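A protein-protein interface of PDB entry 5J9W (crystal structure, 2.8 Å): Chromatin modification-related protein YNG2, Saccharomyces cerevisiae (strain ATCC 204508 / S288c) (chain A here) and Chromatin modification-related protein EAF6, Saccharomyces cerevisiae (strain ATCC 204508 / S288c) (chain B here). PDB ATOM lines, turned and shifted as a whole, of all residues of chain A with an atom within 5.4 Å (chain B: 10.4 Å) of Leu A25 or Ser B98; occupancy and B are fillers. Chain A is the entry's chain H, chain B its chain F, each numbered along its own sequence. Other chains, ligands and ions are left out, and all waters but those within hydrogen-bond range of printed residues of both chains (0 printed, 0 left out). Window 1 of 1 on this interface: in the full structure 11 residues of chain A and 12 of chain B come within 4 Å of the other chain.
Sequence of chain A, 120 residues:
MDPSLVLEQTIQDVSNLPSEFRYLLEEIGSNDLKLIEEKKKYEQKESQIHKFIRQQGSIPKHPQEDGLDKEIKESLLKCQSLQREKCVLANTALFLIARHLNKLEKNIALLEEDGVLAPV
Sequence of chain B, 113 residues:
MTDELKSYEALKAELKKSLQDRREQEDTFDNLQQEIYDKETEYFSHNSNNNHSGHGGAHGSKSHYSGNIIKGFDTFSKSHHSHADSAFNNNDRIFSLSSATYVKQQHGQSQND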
ATOM      1  N   GLU A  20      18.485  28.353 -15.826  1.00  0.00           N
ATOM      2  CA  GLU A  20      18.492  27.870 -17.203  1.00  0.00           C
ATOM      3  C   GLU A  20      17.961  26.446 -17.295  1.00  0.00           C
ATOM      4  O   GLU A  20      17.271  26.098 -18.259  1.00  0.00           O
ATOM      5  CB  GLU A  20      19.909  27.947 -17.768  1.00  0.00           C
ATOM      6  CG  GLU A  20      20.429  29.361 -17.971  1.00  0.00           C
ATOM      7  CD  GLU A  20      21.946  29.414 -18.035  1.00  0.00           C
ATOM      8  OE1 GLU A  20      22.580  28.344 -17.954  1.00  0.00           O
ATOM      9  OE2 GLU A  20      22.506  30.523 -18.161  1.00  0.00           O
ATOM     10  N   PHE A  21      18.288  25.607 -16.309  1.00  0.00           N
ATOM     11  CA  PHE A  21      17.790  24.235 -16.305  1.00  0.00           C
ATOM     12  C   PHE A  21      16.269  24.200 -16.228  1.00  0.00           C
ATOM     13  O   PHE A  21      15.615  23.476 -16.987  1.00  0.00           O
ATOM     14  CB  PHE A  21      18.415  23.462 -15.144  1.00  0.00           C
ATOM     15  CG  PHE A  21      19.551  22.572 -15.554  1.00  0.00           C
ATOM     16  CD1 PHE A  21      20.662  23.094 -16.198  1.00  0.00           C
ATOM     17  CD2 PHE A  21      19.518  21.217 -15.279  1.00  0.00           C
ATOM     18  CE1 PHE A  21      21.710  22.276 -16.574  1.00  0.00           C
ATOM     19  CE2 PHE A  21      20.563  20.395 -15.649  1.00  0.00           C
ATOM     20  CZ  PHE A  21      21.660  20.924 -16.298  1.00  0.00           C
ATOM     21  N   ARG A  22      15.686  24.987 -15.320  1.00  0.00           N
ATOM     22  CA  ARG A  22      14.230  25.063 -15.234  1.00  0.00           C
ATOM     23  C   ARG A  22      13.634  25.575 -16.537  1.00  0.00           C
ATOM     24  O   ARG A  22      12.623  25.050 -17.019  1.00  0.00           O
ATOM     25  CB  ARG A  22      13.824  25.963 -14.069  1.00  0.00           C
ATOM     26  CG  ARG A  22      13.870  25.291 -12.714  1.00  0.00           C
ATOM     27  CD  ARG A  22      13.356  26.226 -11.636  1.00  0.00           C
ATOM     28  NE  ARG A  22      13.216  25.552 -10.352  1.00  0.00           N
ATOM     29  CZ  ARG A  22      12.122  24.900  -9.975  1.00  0.00           C
ATOM     30  NH1 ARG A  22      11.077  24.840 -10.788  1.00  0.00           N
ATOM     31  NH2 ARG A  22      12.072  24.311  -8.789  1.00  0.00           N
ATOM     32  N   TYR A  23      14.254  26.603 -17.121  1.00  0.00           N
ATOM     33  CA  TYR A  23      13.748  27.190 -18.356  1.00  0.00           C
ATOM     34  C   TYR A  23      13.785  26.182 -19.498  1.00  0.00           C
ATOM     35  O   TYR A  23      12.817  26.044 -20.255  1.00  0.00           O
ATOM     36  CB  TYR A  23      14.573  28.432 -18.690  1.00  0.00           C
ATOM     37  CG  TYR A  23      14.168  29.155 -19.947  1.00  0.00           C
ATOM     38  CD1 TYR A  23      12.912  29.735 -20.069  1.00  0.00           C
ATOM     39  CD2 TYR A  23      15.058  29.282 -21.006  1.00  0.00           C
ATOM     40  CE1 TYR A  23      12.551  30.410 -21.221  1.00  0.00           C
ATOM     41  CE2 TYR A  23      14.707  29.953 -22.157  1.00  0.00           C
ATOM     42  CZ  TYR A  23      13.454  30.515 -22.260  1.00  0.00           C
ATOM     43  OH  TYR A  23      13.101  31.186 -23.405  1.00  0.00           O
ATOM     44  N   LEU A  24      14.903  25.467 -19.635  1.00  0.00           N
ATOM     45  CA  LEU A  24      15.029  24.480 -20.702  1.00  0.00           C
ATOM     46  C   LEU A  24      14.100  23.293 -20.476  1.00  0.00           C
ATOM     47  O   LEU A  24      13.439  22.829 -21.412  1.00  0.00           O
ATOM     48  CB  LEU A  24      16.483  24.017 -20.802  1.00  0.00           C
ATOM     49  CG  LEU A  24      17.495  25.049 -21.307  1.00  0.00           C
ATOM     50  CD1 LEU A  24      18.909  24.603 -20.989  1.00  0.00           C
ATOM     51  CD2 LEU A  24      17.339  25.284 -22.800  1.00  0.00           C
ATOM     52  N   LEU A  25      14.032  22.793 -19.238  1.00  0.00           N
ATOM     53  CA  LEU A  25      13.227  21.608 -18.959  1.00  0.00           C
ATOM     54  C   LEU A  25      11.734  21.880 -19.095  1.00  0.00           C
ATOM     55  O   LEU A  25      10.982  20.991 -19.511  1.00  0.00           O
ATOM     56  CB  LEU A  25      13.549  21.074 -17.565  1.00  0.00           C
ATOM     57  CG  LEU A  25      14.917  20.407 -17.427  1.00  0.00           C
ATOM     58  CD1 LEU A  25      15.205  20.060 -15.979  1.00  0.00           C
ATOM     59  CD2 LEU A  25      14.989  19.161 -18.299  1.00  0.00           C
ATOM     60  N   GLU A  26      11.279  23.093 -18.773  1.00  0.00           N
ATOM     61  CA  GLU A  26       9.857  23.378 -18.921  1.00  0.00           C
ATOM     62  C   GLU A  26       9.482  23.611 -20.377  1.00  0.00           C
ATOM     63  O   GLU A  26       8.306  23.482 -20.732  1.00  0.00           O
ATOM     64  CB  GLU A  26       9.449  24.576 -18.060  1.00  0.00           C
ATOM     65  CG  GLU A  26       9.916  25.923 -18.566  1.00  0.00           C
ATOM     66  CD  GLU A  26       9.551  27.050 -17.618  1.00  0.00           C
ATOM     67  OE1 GLU A  26       8.896  26.776 -16.590  1.00  0.00           O
ATOM     68  OE2 GLU A  26       9.921  28.209 -17.901  1.00  0.00           O
ATOM     69  N   GLU A  27      10.454  23.949 -21.223  1.00  0.00           N
ATOM     70  CA  GLU A  27      10.209  23.992 -22.657  1.00  0.00           C
ATOM     71  C   GLU A  27      10.176  22.586 -23.239  1.00  0.00           C
ATOM     72  O   GLU A  27       9.433  22.329 -24.194  1.00  0.00           O
ATOM     73  CB  GLU A  27      11.277  24.839 -23.351  1.00  0.00           C
ATOM     74  CG  GLU A  27      11.019  26.336 -23.264  1.00  0.00           C
ATOM     75  CD  GLU A  27       9.701  26.739 -23.895  1.00  0.00           C
ATOM     76  OE1 GLU A  27       9.476  26.379 -25.071  1.00  0.00           O
ATOM     77  OE2 GLU A  27       8.884  27.396 -23.211  1.00  0.00           O
ATOM     78  N   ILE A  28      10.975  21.673 -22.675  1.00  0.00           N
ATOM     79  CA  ILE A  28      10.899  20.267 -23.063  1.00  0.00           C
ATOM     80  C   ILE A  28       9.542  19.697 -22.682  1.00  0.00           C
ATOM     81  O   ILE A  28       8.911  18.975 -23.464  1.00  0.00           O
ATOM     82  CB  ILE A  28      12.044  19.469 -22.411  1.00  0.00           C
ATOM     83  CG1 ILE A  28      13.404  19.928 -22.933  1.00  0.00           C
ATOM     84  CG2 ILE A  28      11.866  17.981 -22.655  1.00  0.00           C
ATOM     85  CD1 ILE A  28      14.572  19.177 -22.314  1.00  0.00           C
ATOM     86  N   GLY A  29       9.065  20.026 -21.479  1.00  0.00           N
ATOM     87  CA  GLY A  29       7.742  19.587 -21.071  1.00  0.00           C
ATOM     88  C   GLY A  29       6.654  20.194 -21.933  1.00  0.00           C
ATOM     89  O   GLY A  29       5.680  19.526 -22.285  1.00  0.00           O
ATOM     90  N   SER A  30       6.812  21.472 -22.289  1.00  0.00           N
ATOM     91  CA  SER A  30       5.832  22.131 -23.143  1.00  0.00           C
ATOM     92  C   SER A  30       5.761  21.464 -24.513  1.00  0.00           C
ATOM     93  O   SER A  30       4.681  21.360 -25.105  1.00  0.00           O
ATOM     94  CB  SER A  30       6.177  23.614 -23.278  1.00  0.00           C
ATOM     95  OG  SER A  30       5.242  24.283 -24.105  1.00  0.00           O
ATOM     96  N   ASP A  32       6.789  18.208 -25.095  1.00  0.00           N
ATOM     97  CA  ASP A  32       6.337  16.834 -24.912  1.00  0.00           C
ATOM     98  C   ASP A  32       4.821  16.765 -24.799  1.00  0.00           C
ATOM     99  O   ASP A  32       4.209  15.790 -25.250  1.00  0.00           O
ATOM    100  CB  ASP A  32       6.996  16.221 -23.677  1.00  0.00           C
ATOM    101  CG  ASP A  32       6.896  14.708 -23.653  1.00  0.00           C
ATOM    102  OD1 ASP A  32       6.995  14.083 -24.730  1.00  0.00           O
ATOM    103  OD2 ASP A  32       6.709  14.143 -22.556  1.00  0.00           O
ATOM    104  N   PHE B  29      13.314   3.365 -22.726  1.00  0.00           N
ATOM    105  CA  PHE B  29      12.637   4.609 -22.373  1.00  0.00           C
ATOM    106  C   PHE B  29      11.985   4.501 -21.001  1.00  0.00           C
ATOM    107  O   PHE B  29      12.090   5.419 -20.177  1.00  0.00           O
ATOM    108  CB  PHE B  29      11.599   4.955 -23.439  1.00  0.00           C
ATOM    109  CG  PHE B  29      10.712   6.113 -23.078  1.00  0.00           C
ATOM    110  CD1 PHE B  29      11.132   7.419 -23.279  1.00  0.00           C
ATOM    111  CD2 PHE B  29       9.455   5.894 -22.541  1.00  0.00           C
ATOM    112  CE1 PHE B  29      10.312   8.481 -22.952  1.00  0.00           C
ATOM    113  CE2 PHE B  29       8.634   6.951 -22.208  1.00  0.00           C
ATOM    114  CZ  PHE B  29       9.061   8.246 -22.414  1.00  0.00           C
ATOM    115  N   GLN B  33      12.899   6.711 -17.555  1.00  0.00           N
ATOM    116  CA  GLN B  33      11.878   7.413 -16.782  1.00  0.00           C
ATOM    117  C   GLN B  33      11.974   7.054 -15.306  1.00  0.00           C
ATOM    118  O   GLN B  33      11.948   7.931 -14.435  1.00  0.00           O
ATOM    119  CB  GLN B  33      10.491   7.068 -17.319  1.00  0.00           C
ATOM    120  CG  GLN B  33      10.160   7.660 -18.677  1.00  0.00           C
ATOM    121  CD  GLN B  33       9.506   9.021 -18.583  1.00  0.00           C
ATOM    122  OE1 GLN B  33      10.080   9.973 -18.042  1.00  0.00           O
ATOM    123  NE2 GLN B  33       8.286   9.119 -19.099  1.00  0.00           N
ATOM    124  N   ILE B  36      15.375   8.332 -13.846  1.00  0.00           N
ATOM    125  CA  ILE B  36      15.322   9.770 -13.594  1.00  0.00           C
ATOM    126  C   ILE B  36      14.600  10.050 -12.281  1.00  0.00           C
ATOM    127  O   ILE B  36      15.067  10.838 -11.449  1.00  0.00           O
ATOM    128  CB  ILE B  36      14.647  10.498 -14.771  1.00  0.00           C
ATOM    129  CG1 ILE B  36      15.563  10.506 -15.993  1.00  0.00           C
ATOM    130  CG2 ILE B  36      14.269  11.924 -14.369  1.00  0.00           C
ATOM    131  CD1 ILE B  36      14.891  10.988 -17.257  1.00  0.00           C
ATOM    132  N   TYR B  37      13.448   9.403 -12.078  1.00  0.00           N
ATOM    133  CA  TYR B  37      12.692   9.609 -10.846  1.00  0.00           C
ATOM    134  C   TYR B  37      13.488   9.160  -9.625  1.00  0.00           C
ATOM    135  O   TYR B  37      13.478   9.833  -8.586  1.00  0.00           O
ATOM    136  CB  TYR B  37      11.357   8.867 -10.923  1.00  0.00           C
ATOM    137  CG  TYR B  37      10.404   9.206  -9.797  1.00  0.00           C
ATOM    138  CD1 TYR B  37       9.501  10.255  -9.921  1.00  0.00           C
ATOM    139  CD2 TYR B  37      10.410   8.482  -8.613  1.00  0.00           C
ATOM    140  CE1 TYR B  37       8.631  10.573  -8.896  1.00  0.00           C
ATOM    141  CE2 TYR B  37       9.545   8.793  -7.582  1.00  0.00           C
ATOM    142  CZ  TYR B  37       8.657   9.840  -7.728  1.00  0.00           C
ATOM    143  OH  TYR B  37       7.789  10.158  -6.705  1.00  0.00           O
ATOM    144  N   GLU B  40      16.378  11.604  -8.876  1.00  0.00           N
ATOM    145  CA  GLU B  40      15.858  12.805  -8.230  1.00  0.00           C
ATOM    146  C   GLU B  40      15.684  12.580  -6.735  1.00  0.00           C
ATOM    147  O   GLU B  40      15.968  13.470  -5.923  1.00  0.00           O
ATOM    148  CB  GLU B  40      14.524  13.209  -8.859  1.00  0.00           C
ATOM    149  CG  GLU B  40      14.616  13.804 -10.251  1.00  0.00           C
ATOM    150  CD  GLU B  40      13.250  14.149 -10.802  1.00  0.00           C
ATOM    151  OE1 GLU B  40      12.305  13.377 -10.540  1.00  0.00           O
ATOM    152  OE2 GLU B  40      13.111  15.185 -11.488  1.00  0.00           O
ATOM    153  N   PHE B  44      18.413  14.488  -4.134  1.00  0.00           N
ATOM    154  CA  PHE B  44      17.756  15.654  -3.550  1.00  0.00           C
ATOM    155  C   PHE B  44      16.933  15.302  -2.313  1.00  0.00           C
ATOM    156  O   PHE B  44      15.915  15.941  -2.038  1.00  0.00           O
ATOM    157  CB  PHE B  44      16.882  16.351  -4.593  1.00  0.00           C
ATOM    158  CG  PHE B  44      17.617  16.719  -5.852  1.00  0.00           C
ATOM    159  CD1 PHE B  44      18.898  17.240  -5.796  1.00  0.00           C
ATOM    160  CD2 PHE B  44      17.025  16.544  -7.093  1.00  0.00           C
ATOM    161  CE1 PHE B  44      19.578  17.579  -6.951  1.00  0.00           C
ATOM    162  CE2 PHE B  44      17.698  16.881  -8.254  1.00  0.00           C
ATOM    163  CZ  PHE B  44      18.977  17.399  -8.182  1.00  0.00           C
ATOM    164  N   ILE B  69      21.052  22.150  -7.834  1.00  0.00           N
ATOM    165  CA  ILE B  69      20.623  22.604  -9.150  1.00  0.00           C
ATOM    166  C   ILE B  69      19.151  22.983  -9.109  1.00  0.00           C
ATOM    167  O   ILE B  69      18.655  23.670 -10.009  1.00  0.00           O
ATOM    168  CB  ILE B  69      20.894  21.513 -10.204  1.00  0.00           C
ATOM    169  CG1 ILE B  69      20.671  22.038 -11.625  1.00  0.00           C
ATOM    170  CG2 ILE B  69      20.002  20.308  -9.961  1.00  0.00           C
ATOM    171  CD1 ILE B  69      21.577  23.181 -12.009  1.00  0.00           C
ATOM    172  N   ILE B  70      18.439  22.544  -8.073  1.00  0.00           N
ATOM    173  CA  ILE B  70      17.028  22.868  -7.912  1.00  0.00           C
ATOM    174  C   ILE B  70      16.834  24.186  -7.165  1.00  0.00           C
ATOM    175  O   ILE B  70      15.876  24.918  -7.444  1.00  0.00           O
ATOM    176  CB  ILE B  70      16.309  21.719  -7.182  1.00  0.00           C
ATOM    177  CG1 ILE B  70      16.671  20.365  -7.799  1.00  0.00           C
ATOM    178  CG2 ILE B  70      14.799  21.929  -7.194  1.00  0.00           C
ATOM    179  CD1 ILE B  70      16.081  20.127  -9.172  1.00  0.00           C
ATOM    180  N   ASN B  90       7.626  17.106  -4.287  1.00  0.00           N
ATOM    181  CA  ASN B  90       7.311  16.394  -5.520  1.00  0.00           C
ATOM    182  C   ASN B  90       7.139  17.333  -6.704  1.00  0.00           C
ATOM    183  O   ASN B  90       7.141  16.869  -7.849  1.00  0.00           O
ATOM    184  CB  ASN B  90       6.047  15.556  -5.339  1.00  0.00           C
ATOM    185  CG  ASN B  90       6.348  14.090  -5.104  1.00  0.00           C
ATOM    186  OD1 ASN B  90       7.395  13.739  -4.560  1.00  0.00           O
ATOM    187  ND2 ASN B  90       5.429  13.225  -5.519  1.00  0.00           N
ATOM    188  N   ASN B  91       6.991  18.632  -6.453  1.00  0.00           N
ATOM    189  CA  ASN B  91       6.871  19.623  -7.510  1.00  0.00           C
ATOM    190  C   ASN B  91       8.224  20.182  -7.924  1.00  0.00           C
ATOM    191  O   ASN B  91       8.297  20.939  -8.898  1.00  0.00           O
ATOM    192  CB  ASN B  91       5.944  20.764  -7.065  1.00  0.00           C
ATOM    193  CG  ASN B  91       5.304  21.489  -8.237  1.00  0.00           C
ATOM    194  OD1 ASN B  91       5.149  20.923  -9.319  1.00  0.00           O
ATOM    195  ND2 ASN B  91       4.929  22.747  -8.025  1.00  0.00           N
ATOM    196  N   ASP B  92       9.287  19.821  -7.209  1.00  0.00           N
ATOM    197  CA  ASP B  92      10.646  20.231  -7.527  1.00  0.00           C
ATOM    198  C   ASP B  92      11.340  19.238  -8.446  1.00  0.00           C
ATOM    199  O   ASP B  92      12.531  19.399  -8.732  1.00  0.00           O
ATOM    200  CB  ASP B  92      11.459  20.398  -6.237  1.00  0.00           C
ATOM    201  CG  ASP B  92      11.028  21.607  -5.421  1.00  0.00           C
ATOM    202  OD1 ASP B  92      10.606  22.616  -6.026  1.00  0.00           O
ATOM    203  OD2 ASP B  92      11.116  21.551  -4.174  1.00  0.00           O
ATOM    204  N   ARG B  93      10.619  18.211  -8.902  1.00  0.00           N
ATOM    205  CA  ARG B  93      11.157  17.199  -9.809  1.00  0.00           C
ATOM    206  C   ARG B  93      11.125  17.718 -11.249  1.00  0.00           C
ATOM    207  O   ARG B  93      10.431  17.197 -12.120  1.00  0.00           O
ATOM    208  CB  ARG B  93      10.368  15.902  -9.675  1.00  0.00           C
ATOM    209  CG  ARG B  93      10.464  15.237  -8.308  1.00  0.00           C
ATOM    210  CD  ARG B  93       9.642  13.956  -8.250  1.00  0.00           C
ATOM    211  NE  ARG B  93       9.767  13.271  -6.964  1.00  0.00           N
ATOM    212  CZ  ARG B  93      10.671  12.332  -6.700  1.00  0.00           C
ATOM    213  NH1 ARG B  93      11.534  11.959  -7.635  1.00  0.00           N
ATOM    214  NH2 ARG B  93      10.710  11.763  -5.502  1.00  0.00           N
ATOM    215  N   ILE B  94      11.900  18.780 -11.481  1.00  0.00           N
ATOM    216  CA  ILE B  94      11.882  19.457 -12.772  1.00  0.00           C
ATOM    217  C   ILE B  94      12.347  18.543 -13.893  1.00  0.00           C
ATOM    218  O   ILE B  94      12.015  18.777 -15.059  1.00  0.00           O
ATOM    219  CB  ILE B  94      12.736  20.740 -12.724  1.00  0.00           C
ATOM    220  CG1 ILE B  94      14.191  20.404 -12.395  1.00  0.00           C
ATOM    221  CG2 ILE B  94      12.168  21.716 -11.706  1.00  0.00           C
ATOM    222  CD1 ILE B  94      15.096  21.608 -12.371  1.00  0.00           C
ATOM    223  N   PHE B  95      13.111  17.496 -13.569  1.00  0.00           N
ATOM    224  CA  PHE B  95      13.563  16.570 -14.599  1.00  0.00           C
ATOM    225  C   PHE B  95      12.444  15.614 -14.990  1.00  0.00           C
ATOM    226  O   PHE B  95      12.205  15.378 -16.180  1.00  0.00           O
ATOM    227  CB  PHE B  95      14.787  15.790 -14.111  1.00  0.00           C
ATOM    228  CG  PHE B  95      15.950  16.660 -13.735  1.00  0.00           C
ATOM    229  CD1 PHE B  95      16.851  17.099 -14.692  1.00  0.00           C
ATOM    230  CD2 PHE B  95      16.144  17.037 -12.418  1.00  0.00           C
ATOM    231  CE1 PHE B  95      17.920  17.904 -14.339  1.00  0.00           C
ATOM    232  CE2 PHE B  95      17.208  17.839 -12.059  1.00  0.00           C
ATOM    233  CZ  PHE B  95      18.098  18.272 -13.020  1.00  0.00           C
ATOM    234  N   SER B  96      11.742  15.065 -13.994  1.00  0.00           N
ATOM    235  CA  SER B  96      10.631  14.162 -14.274  1.00  0.00           C
ATOM    236  C   SER B  96       9.451  14.910 -14.880  1.00  0.00           C
ATOM    237  O   SER B  96       8.753  14.380 -15.753  1.00  0.00           O
ATOM    238  CB  SER B  96      10.211  13.441 -12.994  1.00  0.00           C
ATOM    239  OG  SER B  96      11.231  12.562 -12.551  1.00  0.00           O
ATOM    240  N   LEU B  97       9.221  16.149 -14.442  1.00  0.00           N
ATOM    241  CA  LEU B  97       8.114  16.932 -14.973  1.00  0.00           C
ATOM    242  C   LEU B  97       8.352  17.370 -16.410  1.00  0.00           C
ATOM    243  O   LEU B  97       7.446  17.938 -17.028  1.00  0.00           O
ATOM    244  CB  LEU B  97       7.867  18.151 -14.085  1.00  0.00           C
ATOM    245  CG  LEU B  97       7.293  17.845 -12.700  1.00  0.00           C
ATOM    246  CD1 LEU B  97       7.415  19.055 -11.795  1.00  0.00           C
ATOM    247  CD2 LEU B  97       5.843  17.413 -12.811  1.00  0.00           C
ATOM    248  N   SER B  98       9.545  17.109 -16.955  1.00  0.00           N
ATOM    249  CA  SER B  98       9.809  17.395 -18.356  1.00  0.00           C
ATOM    250  C   SER B  98       9.111  16.399 -19.262  1.00  0.00           C
ATOM    251  O   SER B  98       8.887  16.694 -20.440  1.00  0.00           O
ATOM    252  CB  SER B  98      11.310  17.362 -18.633  1.00  0.00           C
ATOM    253  OG  SER B  98      12.002  18.233 -17.763  1.00  0.00           O
ATOM    254  N   SER B  99       8.790  15.222 -18.738  1.00  0.00           N
ATOM    255  CA  SER B  99       8.036  14.220 -19.467  1.00  0.00           C
ATOM    256  C   SER B  99       6.550  14.417 -19.208  1.00  0.00           C
ATOM    257  O   SER B  99       6.115  14.456 -18.053  1.00  0.00           O
ATOM    258  CB  SER B  99       8.463  12.815 -19.038  1.00  0.00           C
ATOM    259  OG  SER B  99       7.730  11.822 -19.730  1.00  0.00           O
ATOM    260  N   ALA B 100       5.774  14.547 -20.282  1.00  0.00           N
ATOM    261  CA  ALA B 100       4.333  14.668 -20.122  1.00  0.00           C
ATOM    262  C   ALA B 100       3.695  13.322 -19.816  1.00  0.00           C
ATOM    263  O   ALA B 100       2.526  13.276 -19.418  1.00  0.00           O
ATOM    264  CB  ALA B 100       3.710  15.286 -21.375  1.00  0.00           C
ATOM    265  N   THR B 101       4.446  12.233 -19.999  1.00  0.00           N
ATOM    266  CA  THR B 101       3.973  10.916 -19.588  1.00  0.00           C
ATOM    267  C   THR B 101       3.996  10.798 -18.072  1.00  0.00           C
ATOM    268  O   THR B 101       3.113  10.169 -17.473  1.00  0.00           O
ATOM    269  CB  THR B 101       4.836   9.831 -20.232  1.00  0.00           C
ATOM    270  OG1 THR B 101       4.879  10.034 -21.649  1.00  0.00           O
ATOM    271  CG2 THR B 101       4.273   8.446 -19.944  1.00  0.00           C
ATOM    272  N   TYR B 102       5.002  11.406 -17.437  1.00  0.00           N
ATOM    273  CA  TYR B 102       5.074  11.417 -15.982  1.00  0.00           C
ATOM    274  C   TYR B 102       3.990  12.307 -15.388  1.00  0.00           C
ATOM    275  O   TYR B 102       3.508  12.043 -14.280  1.00  0.00           O
ATOM    276  CB  TYR B 102       6.464  11.878 -15.537  1.00  0.00           C
ATOM    277  CG  TYR B 102       6.555  12.260 -14.079  1.00  0.00           C
ATOM    278  CD1 TYR B 102       6.729  11.295 -13.097  1.00  0.00           C
ATOM    279  CD2 TYR B 102       6.460  13.586 -13.684  1.00  0.00           C
ATOM    280  CE1 TYR B 102       6.808  11.641 -11.761  1.00  0.00           C
ATOM    281  CE2 TYR B 102       6.535  13.942 -12.353  1.00  0.00           C
ATOM    282  CZ  TYR B 102       6.710  12.967 -11.396  1.00  0.00           C
ATOM    283  OH  TYR B 102       6.787  13.317 -10.067  1.00  0.00           O
ATOM    284  N   VAL B 103       3.599  13.363 -16.107  1.00  0.00           N
ATOM    285  CA  VAL B 103       2.537  14.241 -15.628  1.00  0.00           C
ATOM    286  C   VAL B 103       1.201  13.507 -15.644  1.00  0.00           C
ATOM    287  O   VAL B 103       0.383  13.659 -14.728  1.00  0.00           O
ATOM    288  CB  VAL B 103       2.497  15.531 -16.470  1.00  0.00           C
ATOM    289  CG1 VAL B 103       1.358  16.443 -16.020  1.00  0.00           C
ATOM    290  CG2 VAL B 103       3.837  16.252 -16.395  1.00  0.00           C
ATOM    291  N   LYS B 104       0.966  12.698 -16.683  1.00  0.00           N
ATOM    292  CA  LYS B 104      -0.250  11.892 -16.747  1.00  0.00           C
ATOM    293  C   LYS B 104      -0.316  10.910 -15.583  1.00  0.00           C
ATOM    294  O   LYS B 104      -1.375  10.729 -14.970  1.00  0.00           O
ATOM    295  CB  LYS B 104      -0.306  11.141 -18.077  1.00  0.00           C
ATOM    296  CG  LYS B 104      -1.166  11.789 -19.147  1.00  0.00           C
ATOM    297  CD  LYS B 104      -1.197  10.912 -20.390  1.00  0.00           C
ATOM    298  CE  LYS B 104      -2.045  11.520 -21.494  1.00  0.00           C
ATOM    299  NZ  LYS B 104      -2.090  10.648 -22.702  1.00  0.00           N
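No residue of chain B comes within 4 Å of Leu A24. Of chain B, only Ile B94 (3.6 Å), Phe B95 (3.6 Å) and Ser B98 (3.2 Å) come within 4 Å of Leu A25. Printed residues of chain A within 4 Å of Ile B69: Phe A21 (3.9 Å). Printed residues of chain A within 4 Å of Asp B92: Arg A22. Of the printed residues of chain A, Phe B95 touches Phe A21 (3.8 Å) and Leu A25 (3.6 Å). Of chain A, only Leu A25, Ile A28, Gly A29 and Asp A32 come within 4 Å of Ser B98. Of the printed residues of chain A, Ser B99 touches Asp A32. Of the printed residues of chain A, Thr B101 touches Asp A32. The nearest residue of chain B that does not touch Leu A25 is Leu B97 (5.3 Å). The nearest residue of chain A that does not touch Ser B98 is Glu A26 (5.0 Å). The nearest printed residue of chain A that does not touch Ile B94 is Phe A21 (4.7 Å).
The side-chain amide nitrogen (NE2) of Gln B33 sits at hydrogen-bond distance from the side-chain hydroxyl (OG) of Ser B99 (2.8 Å). The side-chain carboxylate of Glu B40 is in hydrogen-bond range of the backbone NH of Phe B95. The backbone carbonyl oxygen of Ile B94 lies within hydrogen-bond range of the side-chain hydroxyl of Ser B98, at 2.8 Å. O of Phe B95 is in hydrogen-bond range of OG of Ser B98 (3.3 Å). OG of Ser B99 lies close to N of Thr B101 (3.3 Å).
Ile B69 touches Phe A21 (CG1 to CD2, 3.9 Å). CE1 of Phe B95 touches CD2 of Phe A21 (3.8 Å). Arg A22 touches Ile B70. Arg A22 touches Ile B94 (NH1 to CG2, 3.4 Å). Leu A25 touches Ile B94. CD1 of Phe B95 touches CD1 of Leu A25, 3.6 Å away. O of Ser B98 touches O of Ile A28, at 3.8 Å. Ser B98 touches Asp A32 (O to CB, 3.8 Å). OD2 of Asp A32 touches CA of Ser B99 (3.4 Å). OD2 of Asp A32 touches N of Thr B101 (3.9 Å).
NH2 of Arg A22 is in salt-bridge range of OD1 of Asp B92 (3.6 Å). O of Leu A25 sits close to OG of Ser B98. The backbone NH (N) of Gly A29 lies close to the backbone carbonyl oxygen (O) of Ser B98, 3.5 Å away. The backbone NH (N) of Ala B100 sits at hydrogen-bond distance from the side-chain carboxylate (OD2) of Asp A32 (2.5 Å).
Of the 12 printed residues of chain A, 6 touch a printed residue of chain B. Printed residues of chain A that touch a printed residue of chain B: Phe A21, Arg A22, Leu A25, Ile A28, Gly A29 and Asp A32. Of the 23 printed residues of chain B, 9 touch a printed residue of chain A. Hydrophobic or aromatic side chains of chain B that line the printed part of chain A: Ile B69, Ile B70, Ile B94, Phe B95 and Ala B100.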
